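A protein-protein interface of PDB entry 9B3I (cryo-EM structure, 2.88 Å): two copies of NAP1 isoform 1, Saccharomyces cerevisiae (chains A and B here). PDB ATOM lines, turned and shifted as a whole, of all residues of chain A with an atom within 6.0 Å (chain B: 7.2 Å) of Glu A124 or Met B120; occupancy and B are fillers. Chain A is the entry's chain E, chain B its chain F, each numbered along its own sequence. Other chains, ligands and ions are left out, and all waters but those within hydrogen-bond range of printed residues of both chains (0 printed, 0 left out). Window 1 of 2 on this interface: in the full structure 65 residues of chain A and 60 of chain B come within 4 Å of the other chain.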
ATOM      1  N   GLN A 117     -25.391   4.432  24.948  1.00  0.00           N
ATOM      2  CA  GLN A 117     -25.024   4.221  23.554  1.00  0.00           C
ATOM      3  C   GLN A 117     -25.065   5.526  22.779  1.00  0.00           C
ATOM      4  O   GLN A 117     -24.203   5.783  21.930  1.00  0.00           O
ATOM      5  CB  GLN A 117     -25.959   3.194  22.917  1.00  0.00           C
ATOM      6  CG  GLN A 117     -25.637   1.737  23.234  1.00  0.00           C
ATOM      7  CD  GLN A 117     -24.374   1.217  22.555  1.00  0.00           C
ATOM      8  OE1 GLN A 117     -23.523   1.984  22.102  1.00  0.00           O
ATOM      9  NE2 GLN A 117     -24.253  -0.104  22.483  1.00  0.00           N
ATOM     10  N   GLU A 119     -24.584   8.570  23.993  1.00  0.00           N
ATOM     11  CA  GLU A 119     -23.437   9.373  24.403  1.00  0.00           C
ATOM     12  C   GLU A 119     -22.149   8.855  23.776  1.00  0.00           C
ATOM     13  O   GLU A 119     -21.327   9.639  23.277  1.00  0.00           O
ATOM     14  CB  GLU A 119     -23.323   9.383  25.925  1.00  0.00           C
ATOM     15  CG  GLU A 119     -24.419  10.153  26.640  1.00  0.00           C
ATOM     16  CD  GLU A 119     -24.363  11.658  26.420  1.00  0.00           C
ATOM     17  OE1 GLU A 119     -23.361  12.174  25.877  1.00  0.00           O
ATOM     18  OE2 GLU A 119     -25.337  12.333  26.811  1.00  0.00           O
ATOM     19  N   MET A 120     -21.951   7.538  23.781  1.00  0.00           N
ATOM     20  CA  MET A 120     -20.751   7.007  23.148  1.00  0.00           C
ATOM     21  C   MET A 120     -20.722   7.355  21.670  1.00  0.00           C
ATOM     22  O   MET A 120     -19.764   7.969  21.202  1.00  0.00           O
ATOM     23  CB  MET A 120     -20.649   5.495  23.357  1.00  0.00           C
ATOM     24  CG  MET A 120     -20.434   5.095  24.806  1.00  0.00           C
ATOM     25  SD  MET A 120     -20.253   3.310  24.975  1.00  0.00           S
ATOM     26  CE  MET A 120     -21.940   2.765  24.732  1.00  0.00           C
ATOM     27  N   PHE A 121     -21.797   7.062  20.937  1.00  0.00           N
ATOM     28  CA  PHE A 121     -21.792   7.346  19.504  1.00  0.00           C
ATOM     29  C   PHE A 121     -21.441   8.800  19.241  1.00  0.00           C
ATOM     30  O   PHE A 121     -20.693   9.102  18.302  1.00  0.00           O
ATOM     31  CB  PHE A 121     -23.135   6.986  18.880  1.00  0.00           C
ATOM     32  CG  PHE A 121     -23.390   5.515  18.825  1.00  0.00           C
ATOM     33  CD1 PHE A 121     -22.370   4.616  19.099  1.00  0.00           C
ATOM     34  CD2 PHE A 121     -24.641   5.027  18.512  1.00  0.00           C
ATOM     35  CE1 PHE A 121     -22.596   3.254  19.051  1.00  0.00           C
ATOM     36  CE2 PHE A 121     -24.875   3.666  18.466  1.00  0.00           C
ATOM     37  CZ  PHE A 121     -23.852   2.777  18.736  1.00  0.00           C
ATOM     38  N   GLU A 122     -21.907   9.707  20.105  1.00  0.00           N
ATOM     39  CA  GLU A 122     -21.421  11.083  20.052  1.00  0.00           C
ATOM     40  C   GLU A 122     -19.903  11.133  20.213  1.00  0.00           C
ATOM     41  O   GLU A 122     -19.217  11.876  19.504  1.00  0.00           O
ATOM     42  CB  GLU A 122     -22.118  11.925  21.125  1.00  0.00           C
ATOM     43  CG  GLU A 122     -21.868  13.434  21.024  1.00  0.00           C
ATOM     44  CD  GLU A 122     -20.582  13.866  21.710  1.00  0.00           C
ATOM     45  OE1 GLU A 122     -20.150  13.183  22.666  1.00  0.00           O
ATOM     46  OE2 GLU A 122     -20.003  14.891  21.293  1.00  0.00           O
ATOM     47  N   LEU A 123     -19.357  10.334  21.139  1.00  0.00           N
ATOM     48  CA  LEU A 123     -17.920  10.410  21.421  1.00  0.00           C
ATOM     49  C   LEU A 123     -17.061   9.831  20.285  1.00  0.00           C
ATOM     50  O   LEU A 123     -16.060  10.445  19.888  1.00  0.00           O
ATOM     51  CB  LEU A 123     -17.616   9.713  22.745  1.00  0.00           C
ATOM     52  CG  LEU A 123     -16.159   9.820  23.182  1.00  0.00           C
ATOM     53  CD1 LEU A 123     -15.762  11.281  23.367  1.00  0.00           C
ATOM     54  CD2 LEU A 123     -15.919   9.048  24.461  1.00  0.00           C
ATOM     55  N   GLU A 124     -17.410   8.649  19.760  1.00  0.00           N
ATOM     56  CA  GLU A 124     -16.700   8.167  18.569  1.00  0.00           C
ATOM     57  C   GLU A 124     -16.893   9.084  17.373  1.00  0.00           C
ATOM     58  O   GLU A 124     -15.989   9.198  16.547  1.00  0.00           O
ATOM     59  CB  GLU A 124     -16.999   6.710  18.158  1.00  0.00           C
ATOM     60  CG  GLU A 124     -16.756   5.530  19.137  1.00  0.00           C
ATOM     61  CD  GLU A 124     -17.897   5.149  20.046  1.00  0.00           C
ATOM     62  OE1 GLU A 124     -18.423   6.015  20.733  1.00  0.00           O
ATOM     63  OE2 GLU A 124     -18.275   3.960  20.070  1.00  0.00           O
ATOM     64  N   ASN A 125     -18.044   9.747  17.241  1.00  0.00           N
ATOM     65  CA  ASN A 125     -18.150  10.719  16.155  1.00  0.00           C
ATOM     66  C   ASN A 125     -17.187  11.882  16.365  1.00  0.00           C
ATOM     67  O   ASN A 125     -16.493  12.304  15.428  1.00  0.00           O
ATOM     68  CB  ASN A 125     -19.586  11.220  16.025  1.00  0.00           C
ATOM     69  CG  ASN A 125     -19.796  12.043  14.770  1.00  0.00           C
ATOM     70  OD1 ASN A 125     -19.649  11.546  13.652  1.00  0.00           O
ATOM     71  ND2 ASN A 125     -20.141  13.312  14.950  1.00  0.00           N
ATOM     72  N   LYS A 126     -17.111  12.388  17.600  1.00  0.00           N
ATOM     73  CA  LYS A 126     -16.193  13.474  17.921  1.00  0.00           C
ATOM     74  C   LYS A 126     -14.756  13.095  17.592  1.00  0.00           C
ATOM     75  O   LYS A 126     -14.035  13.853  16.934  1.00  0.00           O
ATOM     76  CB  LYS A 126     -16.319  13.844  19.399  1.00  0.00           C
ATOM     77  CG  LYS A 126     -15.268  14.830  19.892  1.00  0.00           C
ATOM     78  CD  LYS A 126     -15.475  15.158  21.362  1.00  0.00           C
ATOM     79  CE  LYS A 126     -14.386  16.077  21.885  1.00  0.00           C
ATOM     80  NZ  LYS A 126     -14.619  16.474  23.301  1.00  0.00           N
ATOM     81  N   PHE A 127     -14.324  11.914  18.034  1.00  0.00           N
ATOM     82  CA  PHE A 127     -12.951  11.498  17.775  1.00  0.00           C
ATOM     83  C   PHE A 127     -12.733  11.016  16.344  1.00  0.00           C
ATOM     84  O   PHE A 127     -11.591  10.996  15.880  1.00  0.00           O
ATOM     85  CB  PHE A 127     -12.525  10.417  18.767  1.00  0.00           C
ATOM     86  CG  PHE A 127     -12.048  10.967  20.078  1.00  0.00           C
ATOM     87  CD1 PHE A 127     -12.950  11.343  21.060  1.00  0.00           C
ATOM     88  CD2 PHE A 127     -10.696  11.141  20.314  1.00  0.00           C
ATOM     89  CE1 PHE A 127     -12.506  11.861  22.264  1.00  0.00           C
ATOM     90  CE2 PHE A 127     -10.248  11.661  21.511  1.00  0.00           C
ATOM     91  CZ  PHE A 127     -11.153  12.019  22.489  1.00  0.00           C
ATOM     92  N   LEU A 128     -13.792  10.649  15.625  1.00  0.00           N
ATOM     93  CA  LEU A 128     -13.654  10.370  14.203  1.00  0.00           C
ATOM     94  C   LEU A 128     -13.404  11.649  13.424  1.00  0.00           C
ATOM     95  O   LEU A 128     -12.694  11.634  12.410  1.00  0.00           O
ATOM     96  CB  LEU A 128     -14.906   9.660  13.686  1.00  0.00           C
ATOM     97  CG  LEU A 128     -14.926   9.299  12.203  1.00  0.00           C
ATOM     98  CD1 LEU A 128     -13.846   8.282  11.913  1.00  0.00           C
ATOM     99  CD2 LEU A 128     -16.288   8.764  11.796  1.00  0.00           C
ATOM    100  N   GLN A 129     -13.984  12.761  13.880  1.00  0.00           N
ATOM    101  CA  GLN A 129     -13.639  14.053  13.296  1.00  0.00           C
ATOM    102  C   GLN A 129     -12.155  14.359  13.455  1.00  0.00           C
ATOM    103  O   GLN A 129     -11.580  15.079  12.632  1.00  0.00           O
ATOM    104  CB  GLN A 129     -14.486  15.168  13.914  1.00  0.00           C
ATOM    105  CG  GLN A 129     -15.992  14.973  13.784  1.00  0.00           C
ATOM    106  CD  GLN A 129     -16.375  14.091  12.607  1.00  0.00           C
ATOM    107  OE1 GLN A 129     -16.218  14.478  11.449  1.00  0.00           O
ATOM    108  NE2 GLN A 129     -16.877  12.898  12.902  1.00  0.00           N
ATOM    109  N   TYR A 224     -19.829   7.761   9.931  1.00  0.00           N
ATOM    110  CA  TYR A 224     -20.881   7.246  10.795  1.00  0.00           C
ATOM    111  C   TYR A 224     -22.236   7.746  10.315  1.00  0.00           C
ATOM    112  O   TYR A 224     -22.364   8.893   9.873  1.00  0.00           O
ATOM    113  CB  TYR A 224     -20.658   7.676  12.248  1.00  0.00           C
ATOM    114  CG  TYR A 224     -19.803   6.728  13.055  1.00  0.00           C
ATOM    115  CD1 TYR A 224     -20.034   5.360  13.028  1.00  0.00           C
ATOM    116  CD2 TYR A 224     -18.776   7.204  13.860  1.00  0.00           C
ATOM    117  CE1 TYR A 224     -19.259   4.492  13.773  1.00  0.00           C
ATOM    118  CE2 TYR A 224     -17.997   6.345  14.607  1.00  0.00           C
ATOM    119  CZ  TYR A 224     -18.242   4.990  14.560  1.00  0.00           C
ATOM    120  OH  TYR A 224     -17.470   4.124  15.301  1.00  0.00           O
ATOM    121  N   LYS B 114      -5.163   7.252  22.530  1.00  0.00           N
ATOM    122  CA  LYS B 114      -4.987   7.386  23.973  1.00  0.00           C
ATOM    123  C   LYS B 114      -5.984   8.382  24.553  1.00  0.00           C
ATOM    124  O   LYS B 114      -6.632   8.115  25.573  1.00  0.00           O
ATOM    125  CB  LYS B 114      -3.554   7.816  24.290  1.00  0.00           C
ATOM    126  CG  LYS B 114      -3.300   8.091  25.763  1.00  0.00           C
ATOM    127  CD  LYS B 114      -1.880   8.585  25.997  1.00  0.00           C
ATOM    128  CE  LYS B 114      -1.666   8.985  27.448  1.00  0.00           C
ATOM    129  NZ  LYS B 114      -0.306   9.553  27.674  1.00  0.00           N
ATOM    130  N   GLU B 115      -6.120   9.541  23.905  1.00  0.00           N
ATOM    131  CA  GLU B 115      -7.094  10.529  24.364  1.00  0.00           C
ATOM    132  C   GLU B 115      -8.516   9.984  24.270  1.00  0.00           C
ATOM    133  O   GLU B 115      -9.350  10.231  25.152  1.00  0.00           O
ATOM    134  CB  GLU B 115      -6.956  11.820  23.557  1.00  0.00           C
ATOM    135  CG  GLU B 115      -7.866  12.945  24.028  1.00  0.00           C
ATOM    136  CD  GLU B 115      -7.720  14.202  23.195  1.00  0.00           C
ATOM    137  OE1 GLU B 115      -6.604  14.759  23.148  1.00  0.00           O
ATOM    138  OE2 GLU B 115      -8.722  14.634  22.586  1.00  0.00           O
ATOM    139  N   PHE B 116      -8.806   9.249  23.197  1.00  0.00           N
ATOM    140  CA  PHE B 116     -10.106   8.609  23.033  1.00  0.00           C
ATOM    141  C   PHE B 116     -10.401   7.658  24.185  1.00  0.00           C
ATOM    142  O   PHE B 116     -11.506   7.653  24.740  1.00  0.00           O
ATOM    143  CB  PHE B 116     -10.125   7.877  21.690  1.00  0.00           C
ATOM    144  CG  PHE B 116     -11.317   6.994  21.483  1.00  0.00           C
ATOM    145  CD1 PHE B 116     -12.495   7.505  20.972  1.00  0.00           C
ATOM    146  CD2 PHE B 116     -11.243   5.638  21.761  1.00  0.00           C
ATOM    147  CE1 PHE B 116     -13.587   6.688  20.767  1.00  0.00           C
ATOM    148  CE2 PHE B 116     -12.330   4.816  21.559  1.00  0.00           C
ATOM    149  CZ  PHE B 116     -13.502   5.340  21.058  1.00  0.00           C
ATOM    150  N   GLN B 117      -9.416   6.841  24.554  1.00  0.00           N
ATOM    151  CA  GLN B 117      -9.595   5.903  25.655  1.00  0.00           C
ATOM    152  C   GLN B 117      -9.774   6.633  26.977  1.00  0.00           C
ATOM    153  O   GLN B 117     -10.555   6.198  27.828  1.00  0.00           O
ATOM    154  CB  GLN B 117      -8.409   4.943  25.724  1.00  0.00           C
ATOM    155  CG  GLN B 117      -8.421   3.851  24.660  1.00  0.00           C
ATOM    156  CD  GLN B 117      -9.479   2.784  24.893  1.00  0.00           C
ATOM    157  OE1 GLN B 117     -10.352   2.923  25.750  1.00  0.00           O
ATOM    158  NE2 GLN B 117      -9.400   1.704  24.125  1.00  0.00           N
ATOM    159  N   VAL B 118      -9.056   7.741  27.171  1.00  0.00           N
ATOM    160  CA  VAL B 118      -9.226   8.525  28.392  1.00  0.00           C
ATOM    161  C   VAL B 118     -10.650   9.064  28.482  1.00  0.00           C
ATOM    162  O   VAL B 118     -11.298   8.997  29.536  1.00  0.00           O
ATOM    163  CB  VAL B 118      -8.188   9.659  28.452  1.00  0.00           C
ATOM    164  CG1 VAL B 118      -8.504  10.609  29.595  1.00  0.00           C
ATOM    165  CG2 VAL B 118      -6.790   9.088  28.611  1.00  0.00           C
ATOM    166  N   GLU B 119     -11.154   9.608  27.373  1.00  0.00           N
ATOM    167  CA  GLU B 119     -12.517  10.130  27.362  1.00  0.00           C
ATOM    168  C   GLU B 119     -13.535   9.024  27.614  1.00  0.00           C
ATOM    169  O   GLU B 119     -14.500   9.216  28.367  1.00  0.00           O
ATOM    170  CB  GLU B 119     -12.800  10.834  26.036  1.00  0.00           C
ATOM    171  CG  GLU B 119     -12.057  12.149  25.869  1.00  0.00           C
ATOM    172  CD  GLU B 119     -12.556  13.230  26.812  1.00  0.00           C
ATOM    173  OE1 GLU B 119     -13.666  13.079  27.365  1.00  0.00           O
ATOM    174  OE2 GLU B 119     -11.836  14.233  27.000  1.00  0.00           O
ATOM    175  N   MET B 120     -13.337   7.859  26.991  1.00  0.00           N
ATOM    176  CA  MET B 120     -14.241   6.738  27.226  1.00  0.00           C
ATOM    177  C   MET B 120     -14.204   6.282  28.677  1.00  0.00           C
ATOM    178  O   MET B 120     -15.245   5.952  29.250  1.00  0.00           O
ATOM    179  CB  MET B 120     -13.921   5.576  26.287  1.00  0.00           C
ATOM    180  CG  MET B 120     -14.405   5.795  24.870  1.00  0.00           C
ATOM    181  SD  MET B 120     -16.088   5.157  24.729  1.00  0.00           S
ATOM    182  CE  MET B 120     -16.268   5.006  22.962  1.00  0.00           C
ATOM    183  N   PHE B 121     -13.018   6.242  29.287  1.00  0.00           N
ATOM    184  CA  PHE B 121     -12.931   5.858  30.692  1.00  0.00           C
ATOM    185  C   PHE B 121     -13.664   6.850  31.586  1.00  0.00           C
ATOM    186  O   PHE B 121     -14.394   6.451  32.502  1.00  0.00           O
ATOM    187  CB  PHE B 121     -11.467   5.731  31.116  1.00  0.00           C
ATOM    188  CG  PHE B 121     -11.282   5.055  32.443  1.00  0.00           C
ATOM    189  CD1 PHE B 121     -11.670   3.739  32.626  1.00  0.00           C
ATOM    190  CD2 PHE B 121     -10.721   5.737  33.511  1.00  0.00           C
ATOM    191  CE1 PHE B 121     -11.503   3.116  33.849  1.00  0.00           C
ATOM    192  CE2 PHE B 121     -10.551   5.119  34.735  1.00  0.00           C
ATOM    193  CZ  PHE B 121     -10.942   3.807  34.904  1.00  0.00           C
ATOM    194  N   GLU B 122     -13.486   8.150  31.331  1.00  0.00           N
ATOM    195  CA  GLU B 122     -14.174   9.158  32.135  1.00  0.00           C
ATOM    196  C   GLU B 122     -15.689   9.029  31.999  1.00  0.00           C
ATOM    197  O   GLU B 122     -16.424   9.056  32.998  1.00  0.00           O
ATOM    198  CB  GLU B 122     -13.713  10.559  31.729  1.00  0.00           C
ATOM    199  CG  GLU B 122     -12.289  10.895  32.146  1.00  0.00           C
ATOM    200  CD  GLU B 122     -11.935  12.348  31.892  1.00  0.00           C
ATOM    201  OE1 GLU B 122     -12.513  12.946  30.959  1.00  0.00           O
ATOM    202  OE2 GLU B 122     -11.079  12.891  32.621  1.00  0.00           O
ATOM    203  N   LEU B 123     -16.177   8.871  30.766  1.00  0.00           N
ATOM    204  CA  LEU B 123     -17.619   8.780  30.569  1.00  0.00           C
ATOM    205  C   LEU B 123     -18.175   7.467  31.111  1.00  0.00           C
ATOM    206  O   LEU B 123     -19.309   7.431  31.600  1.00  0.00           O
ATOM    207  CB  LEU B 123     -17.959   8.942  29.088  1.00  0.00           C
ATOM    208  CG  LEU B 123     -19.452   9.009  28.771  1.00  0.00           C
ATOM    209  CD1 LEU B 123     -20.056  10.234  29.439  1.00  0.00           C
ATOM    210  CD2 LEU B 123     -19.684   9.044  27.272  1.00  0.00           C
ATOM    211  N   GLU B 124     -17.393   6.388  31.047  1.00  0.00           N
ATOM    212  CA  GLU B 124     -17.811   5.126  31.643  1.00  0.00           C
ATOM    213  C   GLU B 124     -17.911   5.237  33.156  1.00  0.00           C
ATOM    214  O   GLU B 124     -18.818   4.667  33.766  1.00  0.00           O
ATOM    215  CB  GLU B 124     -16.840   4.017  31.242  1.00  0.00           C
ATOM    216  CG  GLU B 124     -17.004   2.725  32.025  1.00  0.00           C
ATOM    217  CD  GLU B 124     -18.395   2.132  31.914  1.00  0.00           C
ATOM    218  OE1 GLU B 124     -19.057   2.334  30.876  1.00  0.00           O
ATOM    219  OE2 GLU B 124     -18.830   1.464  32.876  1.00  0.00           O
ATOM    220  N   ASN B 125     -16.979   5.956  33.783  1.00  0.00           N
ATOM    221  CA  ASN B 125     -17.083   6.185  35.221  1.00  0.00           C
ATOM    222  C   ASN B 125     -18.332   7.000  35.537  1.00  0.00           C
ATOM    223  O   ASN B 125     -19.061   6.694  36.490  1.00  0.00           O
ATOM    224  CB  ASN B 125     -15.808   6.874  35.724  1.00  0.00           C
ATOM    225  CG  ASN B 125     -15.849   7.236  37.212  1.00  0.00           C
ATOM    226  OD1 ASN B 125     -16.857   7.689  37.751  1.00  0.00           O
ATOM    227  ND2 ASN B 125     -14.723   7.018  37.884  1.00  0.00           N
ATOM    228  N   LYS B 126     -18.594   8.038  34.740  1.00  0.00           N
ATOM    229  CA  LYS B 126     -19.817   8.815  34.926  1.00  0.00           C
ATOM    230  C   LYS B 126     -21.049   7.929  34.823  1.00  0.00           C
ATOM    231  O   LYS B 126     -21.965   8.019  35.650  1.00  0.00           O
ATOM    232  CB  LYS B 126     -19.891   9.939  33.895  1.00  0.00           C
ATOM    233  CG  LYS B 126     -21.108  10.829  34.060  1.00  0.00           C
ATOM    234  CD  LYS B 126     -21.108  11.973  33.066  1.00  0.00           C
ATOM    235  CE  LYS B 126     -22.319  12.867  33.277  1.00  0.00           C
ATOM    236  NZ  LYS B 126     -22.315  14.051  32.377  1.00  0.00           N
ATOM    237  N   PHE B 267      -6.936  -1.332  25.828  1.00  0.00           N
ATOM    238  CA  PHE B 267      -6.072  -1.316  26.996  1.00  0.00           C
ATOM    239  C   PHE B 267      -5.320  -2.636  27.125  1.00  0.00           C
ATOM    240  O   PHE B 267      -5.818  -3.702  26.753  1.00  0.00           O
ATOM    241  CB  PHE B 267      -6.887  -1.057  28.262  1.00  0.00           C
ATOM    242  CG  PHE B 267      -7.183   0.394  28.507  1.00  0.00           C
ATOM    243  CD1 PHE B 267      -6.205   1.241  28.999  1.00  0.00           C
ATOM    244  CD2 PHE B 267      -8.442   0.910  28.248  1.00  0.00           C
ATOM    245  CE1 PHE B 267      -6.476   2.577  29.226  1.00  0.00           C
ATOM    246  CE2 PHE B 267      -8.719   2.245  28.473  1.00  0.00           C
ATOM    247  CZ  PHE B 267      -7.735   3.079  28.962  1.00  0.00           C
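O of Met A120 sits close to OE1 of Glu A124 (2.4 Å).
Among the printed residues, merely in contact across the chains: Glu A119 with Leu B123, Leu A123 with Glu B119, Leu A123 with Met B120, Glu A124 with Phe B116, Glu A124 with Met B120, Phe A127 with Glu B115, Phe A127 with Phe B116 and Phe A127 with Glu B119.
Glu A124 touches just these residues of chain B: Phe B116 (3.7 Å) and Met B120 (3.3 Å).
Met B120 touches just these residues of chain A: Leu A123 (3.6 Å) and Glu A124 (3.3 Å).
Printed residues of chain A within 4 Å of Glu B119: Leu A123 and Phe A127.
Printed residues of chain B within 4 Å of Phe A127: Glu B115 (3.5 Å), Phe B116 (3.3 Å) and Glu B119 (3.5 Å).
Asn B125 touches none of the printed residues of chain A.
Gln A129 touches none of the printed residues of chain B.
The nearest residue of chain A that does not touch Met B120 is Met A120 (4.3 Å).
Of the 13 printed residues of chain A, 4 touch a printed residue of chain B.
Of the 14 printed residues of chain B, 5 touch a printed residue of chain A.
Hydrophobic or aromatic side chains of chain B that line the printed part of chain A: Phe B116, Met B120 and Leu B123.
Among the printed residues, no Asp or Glu carboxylate lies within 4 Å of a Lys or Arg side-chain nitrogen of the other chain.
Glu A119 touches Leu B123, and with the chains exchanged Leu A123 touches Glu B119.
Leu A123 touches Met B120, but with the chains exchanged Met A120 does not touch Leu B123 (4.4 Å).
Glu A124 touches Met B120, but with the chains exchanged Met A120 does not touch Glu B124 (6.1 Å).
Positions printed for both chains: 117, 119, 120, 121, 122, 123, 124, 125 and 126.
Of the 8 pairs that touch across the chains among the printed residues, 2 have their exchanged pair printed and touching as well.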
